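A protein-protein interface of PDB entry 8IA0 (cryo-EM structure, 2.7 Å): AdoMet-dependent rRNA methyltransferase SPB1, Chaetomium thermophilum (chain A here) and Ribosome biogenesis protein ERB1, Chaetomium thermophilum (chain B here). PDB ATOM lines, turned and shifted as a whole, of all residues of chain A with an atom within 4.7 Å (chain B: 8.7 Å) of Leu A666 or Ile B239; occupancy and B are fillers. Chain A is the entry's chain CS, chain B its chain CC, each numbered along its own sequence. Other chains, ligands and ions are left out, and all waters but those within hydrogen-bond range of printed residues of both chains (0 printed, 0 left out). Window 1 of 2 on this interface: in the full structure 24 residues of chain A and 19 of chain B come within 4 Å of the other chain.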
ATOM      1  N   ALA A 659     -10.910 -11.756  30.290  1.00  0.00           N
ATOM      2  CA  ALA A 659     -11.661 -12.336  29.180  1.00  0.00           C
ATOM      3  C   ALA A 659     -10.790 -13.280  28.361  1.00  0.00           C
ATOM      4  O   ALA A 659     -11.246 -14.349  27.939  1.00  0.00           O
ATOM      5  CB  ALA A 659     -12.233 -11.229  28.297  1.00  0.00           C
ATOM      6  N   LEU A 662     -10.433 -16.684  30.240  1.00  0.00           N
ATOM      7  CA  LEU A 662     -11.564 -17.594  30.089  1.00  0.00           C
ATOM      8  C   LEU A 662     -11.588 -18.216  28.700  1.00  0.00           C
ATOM      9  O   LEU A 662     -11.937 -19.391  28.546  1.00  0.00           O
ATOM     10  CB  LEU A 662     -12.872 -16.857  30.370  1.00  0.00           C
ATOM     11  CG  LEU A 662     -14.011 -17.698  30.943  1.00  0.00           C
ATOM     12  CD1 LEU A 662     -13.680 -18.177  32.346  1.00  0.00           C
ATOM     13  CD2 LEU A 662     -15.299 -16.904  30.927  1.00  0.00           C
ATOM     14  N   ALA A 663     -11.230 -17.439  27.676  1.00  0.00           N
ATOM     15  CA  ALA A 663     -11.161 -17.980  26.324  1.00  0.00           C
ATOM     16  C   ALA A 663     -10.067 -19.033  26.208  1.00  0.00           C
ATOM     17  O   ALA A 663     -10.238 -20.041  25.514  1.00  0.00           O
ATOM     18  CB  ALA A 663     -10.933 -16.852  25.321  1.00  0.00           C
ATOM     19  N   HIS A 664      -8.931 -18.810  26.872  1.00  0.00           N
ATOM     20  CA  HIS A 664      -7.859 -19.799  26.859  1.00  0.00           C
ATOM     21  C   HIS A 664      -8.297 -21.093  27.531  1.00  0.00           C
ATOM     22  O   HIS A 664      -7.914 -22.187  27.098  1.00  0.00           O
ATOM     23  CB  HIS A 664      -6.617 -19.235  27.546  1.00  0.00           C
ATOM     24  CG  HIS A 664      -5.701 -18.494  26.624  1.00  0.00           C
ATOM     25  ND1 HIS A 664      -4.341 -18.706  26.599  1.00  0.00           N
ATOM     26  CD2 HIS A 664      -5.951 -17.551  25.688  1.00  0.00           C
ATOM     27  CE1 HIS A 664      -3.791 -17.919  25.692  1.00  0.00           C
ATOM     28  NE2 HIS A 664      -4.748 -17.209  25.123  1.00  0.00           N
ATOM     29  N   GLN A 665      -9.096 -20.989  28.592  1.00  0.00           N
ATOM     30  CA  GLN A 665      -9.579 -22.184  29.273  1.00  0.00           C
ATOM     31  C   GLN A 665     -10.563 -22.969  28.412  1.00  0.00           C
ATOM     32  O   GLN A 665     -10.660 -24.192  28.551  1.00  0.00           O
ATOM     33  CB  GLN A 665     -10.217 -21.802  30.608  1.00  0.00           C
ATOM     34  CG  GLN A 665      -9.280 -21.071  31.552  1.00  0.00           C
ATOM     35  CD  GLN A 665      -9.755 -21.098  32.989  1.00  0.00           C
ATOM     36  OE1 GLN A 665     -10.807 -20.552  33.316  1.00  0.00           O
ATOM     37  NE2 GLN A 665      -8.978 -21.732  33.857  1.00  0.00           N
ATOM     38  N   LEU A 666     -11.308 -22.292  27.535  1.00  0.00           N
ATOM     39  CA  LEU A 666     -12.179 -23.011  26.608  1.00  0.00           C
ATOM     40  C   LEU A 666     -11.384 -23.664  25.486  1.00  0.00           C
ATOM     41  O   LEU A 666     -11.667 -24.805  25.104  1.00  0.00           O
ATOM     42  CB  LEU A 666     -13.234 -22.074  26.024  1.00  0.00           C
ATOM     43  CG  LEU A 666     -14.626 -22.132  26.651  1.00  0.00           C
ATOM     44  CD1 LEU A 666     -15.591 -21.277  25.855  1.00  0.00           C
ATOM     45  CD2 LEU A 666     -15.120 -23.564  26.726  1.00  0.00           C
ATOM     46  N   ALA A 667     -10.397 -22.953  24.934  1.00  0.00           N
ATOM     47  CA  ALA A 667      -9.589 -23.517  23.857  1.00  0.00           C
ATOM     48  C   ALA A 667      -8.861 -24.771  24.320  1.00  0.00           C
ATOM     49  O   ALA A 667      -8.877 -25.802  23.639  1.00  0.00           O
ATOM     50  CB  ALA A 667      -8.598 -22.471  23.346  1.00  0.00           C
ATOM     51  N   THR A 668      -8.219 -24.701  25.480  1.00  0.00           N
ATOM     52  CA  THR A 668      -7.664 -25.890  26.103  1.00  0.00           C
ATOM     53  C   THR A 668      -8.790 -26.748  26.672  1.00  0.00           C
ATOM     54  O   THR A 668      -9.899 -26.269  26.925  1.00  0.00           O
ATOM     55  CB  THR A 668      -6.683 -25.501  27.208  1.00  0.00           C
ATOM     56  OG1 THR A 668      -5.921 -24.364  26.787  1.00  0.00           O
ATOM     57  CG2 THR A 668      -5.725 -26.644  27.509  1.00  0.00           C
ATOM     58  N   LYS A 671     -11.894 -26.334  30.906  1.00  0.00           N
ATOM     59  CA  LYS A 671     -13.307 -26.300  31.237  1.00  0.00           C
ATOM     60  C   LYS A 671     -14.118 -26.289  29.950  1.00  0.00           C
ATOM     61  O   LYS A 671     -13.782 -25.590  28.991  1.00  0.00           O
ATOM     62  CB  LYS A 671     -13.664 -25.084  32.098  1.00  0.00           C
ATOM     63  CG  LYS A 671     -12.932 -23.817  31.720  1.00  0.00           C
ATOM     64  CD  LYS A 671     -13.441 -22.624  32.514  1.00  0.00           C
ATOM     65  CE  LYS A 671     -13.467 -22.904  34.010  1.00  0.00           C
ATOM     66  NZ  LYS A 671     -12.191 -23.494  34.503  1.00  0.00           N
ATOM     67  N   THR A 672     -15.187 -27.072  29.939  1.00  0.00           N
ATOM     68  CA  THR A 672     -16.034 -27.249  28.770  1.00  0.00           C
ATOM     69  C   THR A 672     -17.140 -26.201  28.759  1.00  0.00           C
ATOM     70  O   THR A 672     -17.219 -25.332  29.632  1.00  0.00           O
ATOM     71  CB  THR A 672     -16.617 -28.663  28.743  1.00  0.00           C
ATOM     72  OG1 THR A 672     -17.160 -28.981  30.030  1.00  0.00           O
ATOM     73  CG2 THR A 672     -15.538 -29.676  28.392  1.00  0.00           C
ATOM     74  N   LYS A 673     -17.999 -26.285  27.741  1.00  0.00           N
ATOM     75  CA  LYS A 673     -19.118 -25.355  27.637  1.00  0.00           C
ATOM     76  C   LYS A 673     -20.092 -25.536  28.794  1.00  0.00           C
ATOM     77  O   LYS A 673     -20.641 -24.557  29.312  1.00  0.00           O
ATOM     78  CB  LYS A 673     -19.833 -25.539  26.300  1.00  0.00           C
ATOM     79  CG  LYS A 673     -19.383 -24.569  25.216  1.00  0.00           C
ATOM     80  CD  LYS A 673     -19.855 -24.962  23.809  1.00  0.00           C
ATOM     81  CE  LYS A 673     -21.309 -25.454  23.717  1.00  0.00           C
ATOM     82  NZ  LYS A 673     -22.280 -24.853  24.683  1.00  0.00           N
ATOM     83  N   LEU A 676     -18.786 -23.773  31.987  1.00  0.00           N
ATOM     84  CA  LEU A 676     -18.912 -22.319  32.005  1.00  0.00           C
ATOM     85  C   LEU A 676     -20.334 -21.883  32.335  1.00  0.00           C
ATOM     86  O   LEU A 676     -20.533 -20.878  33.029  1.00  0.00           O
ATOM     87  CB  LEU A 676     -18.469 -21.734  30.666  1.00  0.00           C
ATOM     88  CG  LEU A 676     -16.978 -21.423  30.546  1.00  0.00           C
ATOM     89  CD1 LEU A 676     -16.706 -20.611  29.296  1.00  0.00           C
ATOM     90  CD2 LEU A 676     -16.486 -20.687  31.777  1.00  0.00           C
ATOM     91  N   THR B 218      -6.647 -16.295  19.706  1.00  0.00           N
ATOM     92  CA  THR B 218      -6.267 -16.551  21.089  1.00  0.00           C
ATOM     93  C   THR B 218      -4.768 -16.605  21.325  1.00  0.00           C
ATOM     94  O   THR B 218      -4.348 -16.494  22.482  1.00  0.00           O
ATOM     95  CB  THR B 218      -6.878 -17.871  21.584  1.00  0.00           C
ATOM     96  OG1 THR B 218      -6.428 -18.947  20.751  1.00  0.00           O
ATOM     97  CG2 THR B 218      -8.388 -17.809  21.544  1.00  0.00           C
ATOM     98  N   LEU B 220      -2.984 -19.270  20.890  1.00  0.00           N
ATOM     99  CA  LEU B 220      -2.664 -20.651  21.214  1.00  0.00           C
ATOM    100  C   LEU B 220      -2.512 -21.472  19.938  1.00  0.00           C
ATOM    101  O   LEU B 220      -2.903 -21.055  18.846  1.00  0.00           O
ATOM    102  CB  LEU B 220      -3.750 -21.253  22.110  1.00  0.00           C
ATOM    103  CG  LEU B 220      -3.809 -20.763  23.556  1.00  0.00           C
ATOM    104  CD1 LEU B 220      -4.893 -21.500  24.323  1.00  0.00           C
ATOM    105  CD2 LEU B 220      -2.460 -20.934  24.232  1.00  0.00           C
ATOM    106  N   LEU B 229      -5.315 -21.969  17.112  1.00  0.00           N
ATOM    107  CA  LEU B 229      -6.650 -22.254  17.612  1.00  0.00           C
ATOM    108  C   LEU B 229      -7.464 -20.970  17.661  1.00  0.00           C
ATOM    109  O   LEU B 229      -7.047 -19.986  18.281  1.00  0.00           O
ATOM    110  CB  LEU B 229      -6.579 -22.889  18.999  1.00  0.00           C
ATOM    111  CG  LEU B 229      -7.517 -24.060  19.292  1.00  0.00           C
ATOM    112  CD1 LEU B 229      -7.225 -24.624  20.669  1.00  0.00           C
ATOM    113  CD2 LEU B 229      -8.974 -23.641  19.182  1.00  0.00           C
ATOM    114  N   ASN B 230      -8.621 -20.984  17.010  1.00  0.00           N
ATOM    115  CA  ASN B 230      -9.509 -19.834  16.959  1.00  0.00           C
ATOM    116  C   ASN B 230     -10.859 -20.199  17.557  1.00  0.00           C
ATOM    117  O   ASN B 230     -11.394 -21.279  17.292  1.00  0.00           O
ATOM    118  CB  ASN B 230      -9.690 -19.338  15.522  1.00  0.00           C
ATOM    119  CG  ASN B 230      -8.584 -18.400  15.087  1.00  0.00           C
ATOM    120  OD1 ASN B 230      -7.527 -18.337  15.714  1.00  0.00           O
ATOM    121  ND2 ASN B 230      -8.823 -17.663  14.008  1.00  0.00           N
ATOM    122  N   LEU B 231     -11.401 -19.295  18.366  1.00  0.00           N
ATOM    123  CA  LEU B 231     -12.737 -19.485  18.901  1.00  0.00           C
ATOM    124  C   LEU B 231     -13.778 -19.304  17.801  1.00  0.00           C
ATOM    125  O   LEU B 231     -13.539 -18.659  16.778  1.00  0.00           O
ATOM    126  CB  LEU B 231     -13.013 -18.500  20.036  1.00  0.00           C
ATOM    127  CG  LEU B 231     -12.190 -18.622  21.315  1.00  0.00           C
ATOM    128  CD1 LEU B 231     -11.878 -17.237  21.849  1.00  0.00           C
ATOM    129  CD2 LEU B 231     -12.927 -19.442  22.354  1.00  0.00           C
ATOM    130  N   SER B 232     -14.948 -19.889  18.024  1.00  0.00           N
ATOM    131  CA  SER B 232     -16.062 -19.762  17.101  1.00  0.00           C
ATOM    132  C   SER B 232     -17.063 -18.744  17.640  1.00  0.00           C
ATOM    133  O   SER B 232     -16.914 -18.207  18.740  1.00  0.00           O
ATOM    134  CB  SER B 232     -16.717 -21.124  16.866  1.00  0.00           C
ATOM    135  OG  SER B 232     -17.268 -21.638  18.065  1.00  0.00           O
ATOM    136  N   ARG B 233     -18.098 -18.468  16.843  1.00  0.00           N
ATOM    137  CA  ARG B 233     -19.079 -17.459  17.226  1.00  0.00           C
ATOM    138  C   ARG B 233     -19.853 -17.877  18.469  1.00  0.00           C
ATOM    139  O   ARG B 233     -20.115 -17.056  19.355  1.00  0.00           O
ATOM    140  CB  ARG B 233     -20.034 -17.186  16.063  1.00  0.00           C
ATOM    141  CG  ARG B 233     -19.497 -16.207  15.031  1.00  0.00           C
ATOM    142  CD  ARG B 233     -19.142 -14.860  15.649  1.00  0.00           C
ATOM    143  NE  ARG B 233     -20.080 -14.460  16.693  1.00  0.00           N
ATOM    144  CZ  ARG B 233     -20.678 -13.279  16.749  1.00  0.00           C
ATOM    145  NH1 ARG B 233     -20.456 -12.348  15.835  1.00  0.00           N
ATOM    146  NH2 ARG B 233     -21.519 -13.024  17.746  1.00  0.00           N
ATOM    147  N   ASP B 234     -20.236 -19.153  18.550  1.00  0.00           N
ATOM    148  CA  ASP B 234     -20.979 -19.618  19.716  1.00  0.00           C
ATOM    149  C   ASP B 234     -20.128 -19.537  20.976  1.00  0.00           C
ATOM    150  O   ASP B 234     -20.637 -19.211  22.055  1.00  0.00           O
ATOM    151  CB  ASP B 234     -21.483 -21.043  19.496  1.00  0.00           C
ATOM    152  CG  ASP B 234     -20.402 -21.974  18.992  1.00  0.00           C
ATOM    153  OD1 ASP B 234     -19.499 -21.499  18.274  1.00  0.00           O
ATOM    154  OD2 ASP B 234     -20.453 -23.180  19.314  1.00  0.00           O
ATOM    155  N   GLU B 235     -18.832 -19.831  20.861  1.00  0.00           N
ATOM    156  CA  GLU B 235     -17.950 -19.717  22.017  1.00  0.00           C
ATOM    157  C   GLU B 235     -17.782 -18.263  22.441  1.00  0.00           C
ATOM    158  O   GLU B 235     -17.811 -17.957  23.637  1.00  0.00           O
ATOM    159  CB  GLU B 235     -16.594 -20.348  21.709  1.00  0.00           C
ATOM    160  CG  GLU B 235     -16.673 -21.803  21.291  1.00  0.00           C
ATOM    161  CD  GLU B 235     -15.371 -22.541  21.517  1.00  0.00           C
ATOM    162  OE1 GLU B 235     -14.636 -22.172  22.455  1.00  0.00           O
ATOM    163  OE2 GLU B 235     -15.081 -23.486  20.754  1.00  0.00           O
ATOM    164  N   LEU B 236     -17.631 -17.352  21.477  1.00  0.00           N
ATOM    165  CA  LEU B 236     -17.449 -15.941  21.813  1.00  0.00           C
ATOM    166  C   LEU B 236     -18.670 -15.383  22.531  1.00  0.00           C
ATOM    167  O   LEU B 236     -18.541 -14.544  23.429  1.00  0.00           O
ATOM    168  CB  LEU B 236     -17.156 -15.131  20.551  1.00  0.00           C
ATOM    169  CG  LEU B 236     -15.768 -15.306  19.937  1.00  0.00           C
ATOM    170  CD1 LEU B 236     -15.812 -15.024  18.450  1.00  0.00           C
ATOM    171  CD2 LEU B 236     -14.760 -14.402  20.625  1.00  0.00           C
ATOM    172  N   GLU B 237     -19.863 -15.831  22.140  1.00  0.00           N
ATOM    173  CA  GLU B 237     -21.071 -15.430  22.851  1.00  0.00           C
ATOM    174  C   GLU B 237     -21.050 -15.927  24.289  1.00  0.00           C
ATOM    175  O   GLU B 237     -21.509 -15.231  25.201  1.00  0.00           O
ATOM    176  CB  GLU B 237     -22.306 -15.955  22.117  1.00  0.00           C
ATOM    177  CG  GLU B 237     -22.590 -15.279  20.781  1.00  0.00           C
ATOM    178  CD  GLU B 237     -22.835 -13.783  20.896  1.00  0.00           C
ATOM    179  OE1 GLU B 237     -23.133 -13.298  22.009  1.00  0.00           O
ATOM    180  OE2 GLU B 237     -22.729 -13.088  19.864  1.00  0.00           O
ATOM    181  N   LEU B 238     -20.526 -17.135  24.510  1.00  0.00           N
ATOM    182  CA  LEU B 238     -20.475 -17.688  25.858  1.00  0.00           C
ATOM    183  C   LEU B 238     -19.549 -16.880  26.761  1.00  0.00           C
ATOM    184  O   LEU B 238     -19.873 -16.632  27.928  1.00  0.00           O
ATOM    185  CB  LEU B 238     -20.040 -19.151  25.804  1.00  0.00           C
ATOM    186  CG  LEU B 238     -20.106 -19.928  27.118  1.00  0.00           C
ATOM    187  CD1 LEU B 238     -21.546 -20.044  27.584  1.00  0.00           C
ATOM    188  CD2 LEU B 238     -19.488 -21.302  26.948  1.00  0.00           C
ATOM    189  N   ILE B 239     -18.387 -16.467  26.247  1.00  0.00           N
ATOM    190  CA  ILE B 239     -17.504 -15.598  27.023  1.00  0.00           C
ATOM    191  C   ILE B 239     -18.173 -14.256  27.286  1.00  0.00           C
ATOM    192  O   ILE B 239     -18.070 -13.701  28.387  1.00  0.00           O
ATOM    193  CB  ILE B 239     -16.140 -15.425  26.322  1.00  0.00           C
ATOM    194  CG1 ILE B 239     -15.254 -16.656  26.523  1.00  0.00           C
ATOM    195  CG2 ILE B 239     -15.420 -14.184  26.827  1.00  0.00           C
ATOM    196  CD1 ILE B 239     -15.408 -17.719  25.484  1.00  0.00           C
ATOM    197  N   ARG B 240     -18.868 -13.714  26.285  1.00  0.00           N
ATOM    198  CA  ARG B 240     -19.578 -12.453  26.481  1.00  0.00           C
ATOM    199  C   ARG B 240     -20.652 -12.591  27.550  1.00  0.00           C
ATOM    200  O   ARG B 240     -20.816 -11.704  28.395  1.00  0.00           O
ATOM    201  CB  ARG B 240     -20.196 -11.984  25.166  1.00  0.00           C
ATOM    202  CG  ARG B 240     -20.815 -10.597  25.236  1.00  0.00           C
ATOM    203  CD  ARG B 240     -22.330 -10.662  25.327  1.00  0.00           C
ATOM    204  NE  ARG B 240     -22.959 -10.851  24.027  1.00  0.00           N
ATOM    205  CZ  ARG B 240     -24.174 -10.421  23.717  1.00  0.00           C
ATOM    206  NH1 ARG B 240     -24.923  -9.773  24.594  1.00  0.00           N
ATOM    207  NH2 ARG B 240     -24.649 -10.646  22.495  1.00  0.00           N
ATOM    208  N   LYS B 241     -21.395 -13.699  27.528  1.00  0.00           N
ATOM    209  CA  LYS B 241     -22.447 -13.901  28.516  1.00  0.00           C
ATOM    210  C   LYS B 241     -21.875 -14.030  29.922  1.00  0.00           C
ATOM    211  O   LYS B 241     -22.411 -13.448  30.871  1.00  0.00           O
ATOM    212  CB  LYS B 241     -23.269 -15.140  28.157  1.00  0.00           C
ATOM    213  CG  LYS B 241     -24.602 -14.832  27.501  1.00  0.00           C
ATOM    214  CD  LYS B 241     -24.622 -15.264  26.047  1.00  0.00           C
ATOM    215  CE  LYS B 241     -26.002 -15.085  25.439  1.00  0.00           C
ATOM    216  NZ  LYS B 241     -26.360 -13.649  25.283  1.00  0.00           N
ATOM    217  N   VAL B 242     -20.789 -14.789  30.078  1.00  0.00           N
ATOM    218  CA  VAL B 242     -20.248 -15.033  31.412  1.00  0.00           C
ATOM    219  C   VAL B 242     -19.597 -13.774  31.971  1.00  0.00           C
ATOM    220  O   VAL B 242     -19.819 -13.409  33.132  1.00  0.00           O
ATOM    221  CB  VAL B 242     -19.261 -16.213  31.383  1.00  0.00           C
ATOM    222  CG1 VAL B 242     -18.368 -16.184  32.612  1.00  0.00           C
ATOM    223  CG2 VAL B 242     -20.013 -17.529  31.295  1.00  0.00           C
ATOM    224  N   GLN B 243     -18.792 -13.086  31.159  1.00  0.00           N
ATOM    225  CA  GLN B 243     -18.057 -11.926  31.650  1.00  0.00           C
ATOM    226  C   GLN B 243     -18.974 -10.777  32.041  1.00  0.00           C
ATOM    227  O   GLN B 243     -18.588  -9.950  32.872  1.00  0.00           O
ATOM    228  CB  GLN B 243     -17.049 -11.460  30.601  1.00  0.00           C
ATOM    229  CG  GLN B 243     -15.913 -10.634  31.171  1.00  0.00           C
ATOM    230  CD  GLN B 243     -14.719 -11.478  31.561  1.00  0.00           C
ATOM    231  OE1 GLN B 243     -14.857 -12.658  31.883  1.00  0.00           O
ATOM    232  NE2 GLN B 243     -13.538 -10.874  31.542  1.00  0.00           N
ATOM    233  N   GLN B 244     -20.171 -10.703  31.465  1.00  0.00           N
ATOM    234  CA  GLN B 244     -21.171  -9.737  31.897  1.00  0.00           C
ATOM    235  C   GLN B 244     -22.185 -10.327  32.865  1.00  0.00           C
ATOM    236  O   GLN B 244     -22.726  -9.595  33.699  1.00  0.00           O
ATOM    237  CB  GLN B 244     -21.905  -9.151  30.687  1.00  0.00           C
ATOM    238  CG  GLN B 244     -20.987  -8.716  29.557  1.00  0.00           C
ATOM    239  CD  GLN B 244     -21.748  -8.173  28.366  1.00  0.00           C
ATOM    240  OE1 GLN B 244     -22.704  -8.785  27.894  1.00  0.00           O
ATOM    241  NE2 GLN B 244     -21.321  -7.019  27.868  1.00  0.00           N
ATOM    242  N   GLY B 245     -22.458 -11.626  32.772  1.00  0.00           N
ATOM    243  CA  GLY B 245     -23.361 -12.293  33.684  1.00  0.00           C
ATOM    244  C   GLY B 245     -24.831 -12.066  33.420  1.00  0.00           C
ATOM    245  O   GLY B 245     -25.661 -12.540  34.206  1.00  0.00           O
ATOM    246  N   LEU B 246     -25.183 -11.360  32.344  1.00  0.00           N
ATOM    247  CA  LEU B 246     -26.579 -10.998  32.121  1.00  0.00           C
ATOM    248  C   LEU B 246     -27.442 -12.224  31.842  1.00  0.00           C
ATOM    249  O   LEU B 246     -28.566 -12.323  32.345  1.00  0.00           O
ATOM    250  CB  LEU B 246     -26.682  -9.977  30.983  1.00  0.00           C
ATOM    251  CG  LEU B 246     -26.599 -10.415  29.518  1.00  0.00           C
ATOM    252  CD1 LEU B 246     -27.113  -9.313  28.605  1.00  0.00           C
ATOM    253  CD2 LEU B 246     -25.180 -10.807  29.137  1.00  0.00           C
ATOM    254  N   ILE B 247     -26.941 -13.166  31.048  1.00  0.00           N
ATOM    255  CA  ILE B 247     -27.698 -14.367  30.704  1.00  0.00           C
ATOM    256  C   ILE B 247     -26.819 -15.592  30.921  1.00  0.00           C
ATOM    257  O   ILE B 247     -26.116 -16.022  29.993  1.00  0.00           O
ATOM    258  CB  ILE B 247     -28.223 -14.309  29.259  1.00  0.00           C
ATOM    259  CG1 ILE B 247     -29.080 -13.060  29.045  1.00  0.00           C
ATOM    260  CG2 ILE B 247     -29.043 -15.549  28.936  1.00  0.00           C
ATOM    261  CD1 ILE B 247     -29.521 -12.858  27.611  1.00  0.00           C
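Leu A662 touches Val B242. Ala A663 touches Leu B231 (CB to CD1, 3.6 Å). His A664 touches Leu B220. Leu A666 touches Glu B235. Leu B220 touches Ala A667 (CD1 to CB, 3.95 Å). Ala A667 touches Leu B229 (O to CD1, 3.6 Å). Thr A668 touches Leu B220 (OG1 to CD1, 3.9 Å). Leu B238 touches Lys A673. Leu B238 touches Leu A676 (CD2 to CD1, 3.7 Å). Leu A676 touches Val B242 (O to CG2, 3.8 Å).
Of the printed residues of chain B, Ala A659 touches Gln B243. Ala A663 touches just one residue of chain B: Leu B231. Gln A665 touches none of the printed residues of chain B. Leu A666 touches two residues of chain B. Ala A667 touches just these residues of chain B: Leu B220 (3.95 Å) and Leu B229 (3.6 Å). Of the printed residues of chain B, Lys A673 touches Leu B238 (3.7 Å). Ile B239 touches just one residue of chain A: Leu A666 (3.6 Å). Lys B241 touches none of the printed residues of chain A.
O of Thr B218 lies within hydrogen-bond range of NE2 of His A664 (2.8 Å). NE2 of Gln B243 lies close to N of Ala A659 (3.0 Å).
Hydrophobic or aromatic side chains of chain B within 4 Å of the printed part of chain A: Leu B220, Leu B229, Leu B231, Leu B238, Ile B239 and Val B242. Printed residues of chain A that touch a printed residue of chain B: Ala A659, Leu A662, Ala A663, His A664, Leu A666, Ala A667, Thr A668, Lys A673 and Leu A676. Among the printed residues, no Asp or Glu carboxylate lies within 4 Å of a Lys or Arg side-chain nitrogen of the other chain.
The backbone carbonyl oxygen (O) of His A664 lies within hydrogen-bond range of the side-chain hydroxyl (OG1) of Thr A668, 3.0 Å away. OG1 of Thr B218 lies close to N of Leu B220, 3.5 Å away. The backbone carbonyl oxygen of Leu B229 is in hydrogen-bond range of the side-chain hydroxyl of Thr B218 (2.8 Å). The backbone NH (N) of Leu B229 lies within hydrogen-bond range of the backbone carbonyl oxygen (O) of Leu B220, 3.1 Å away.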
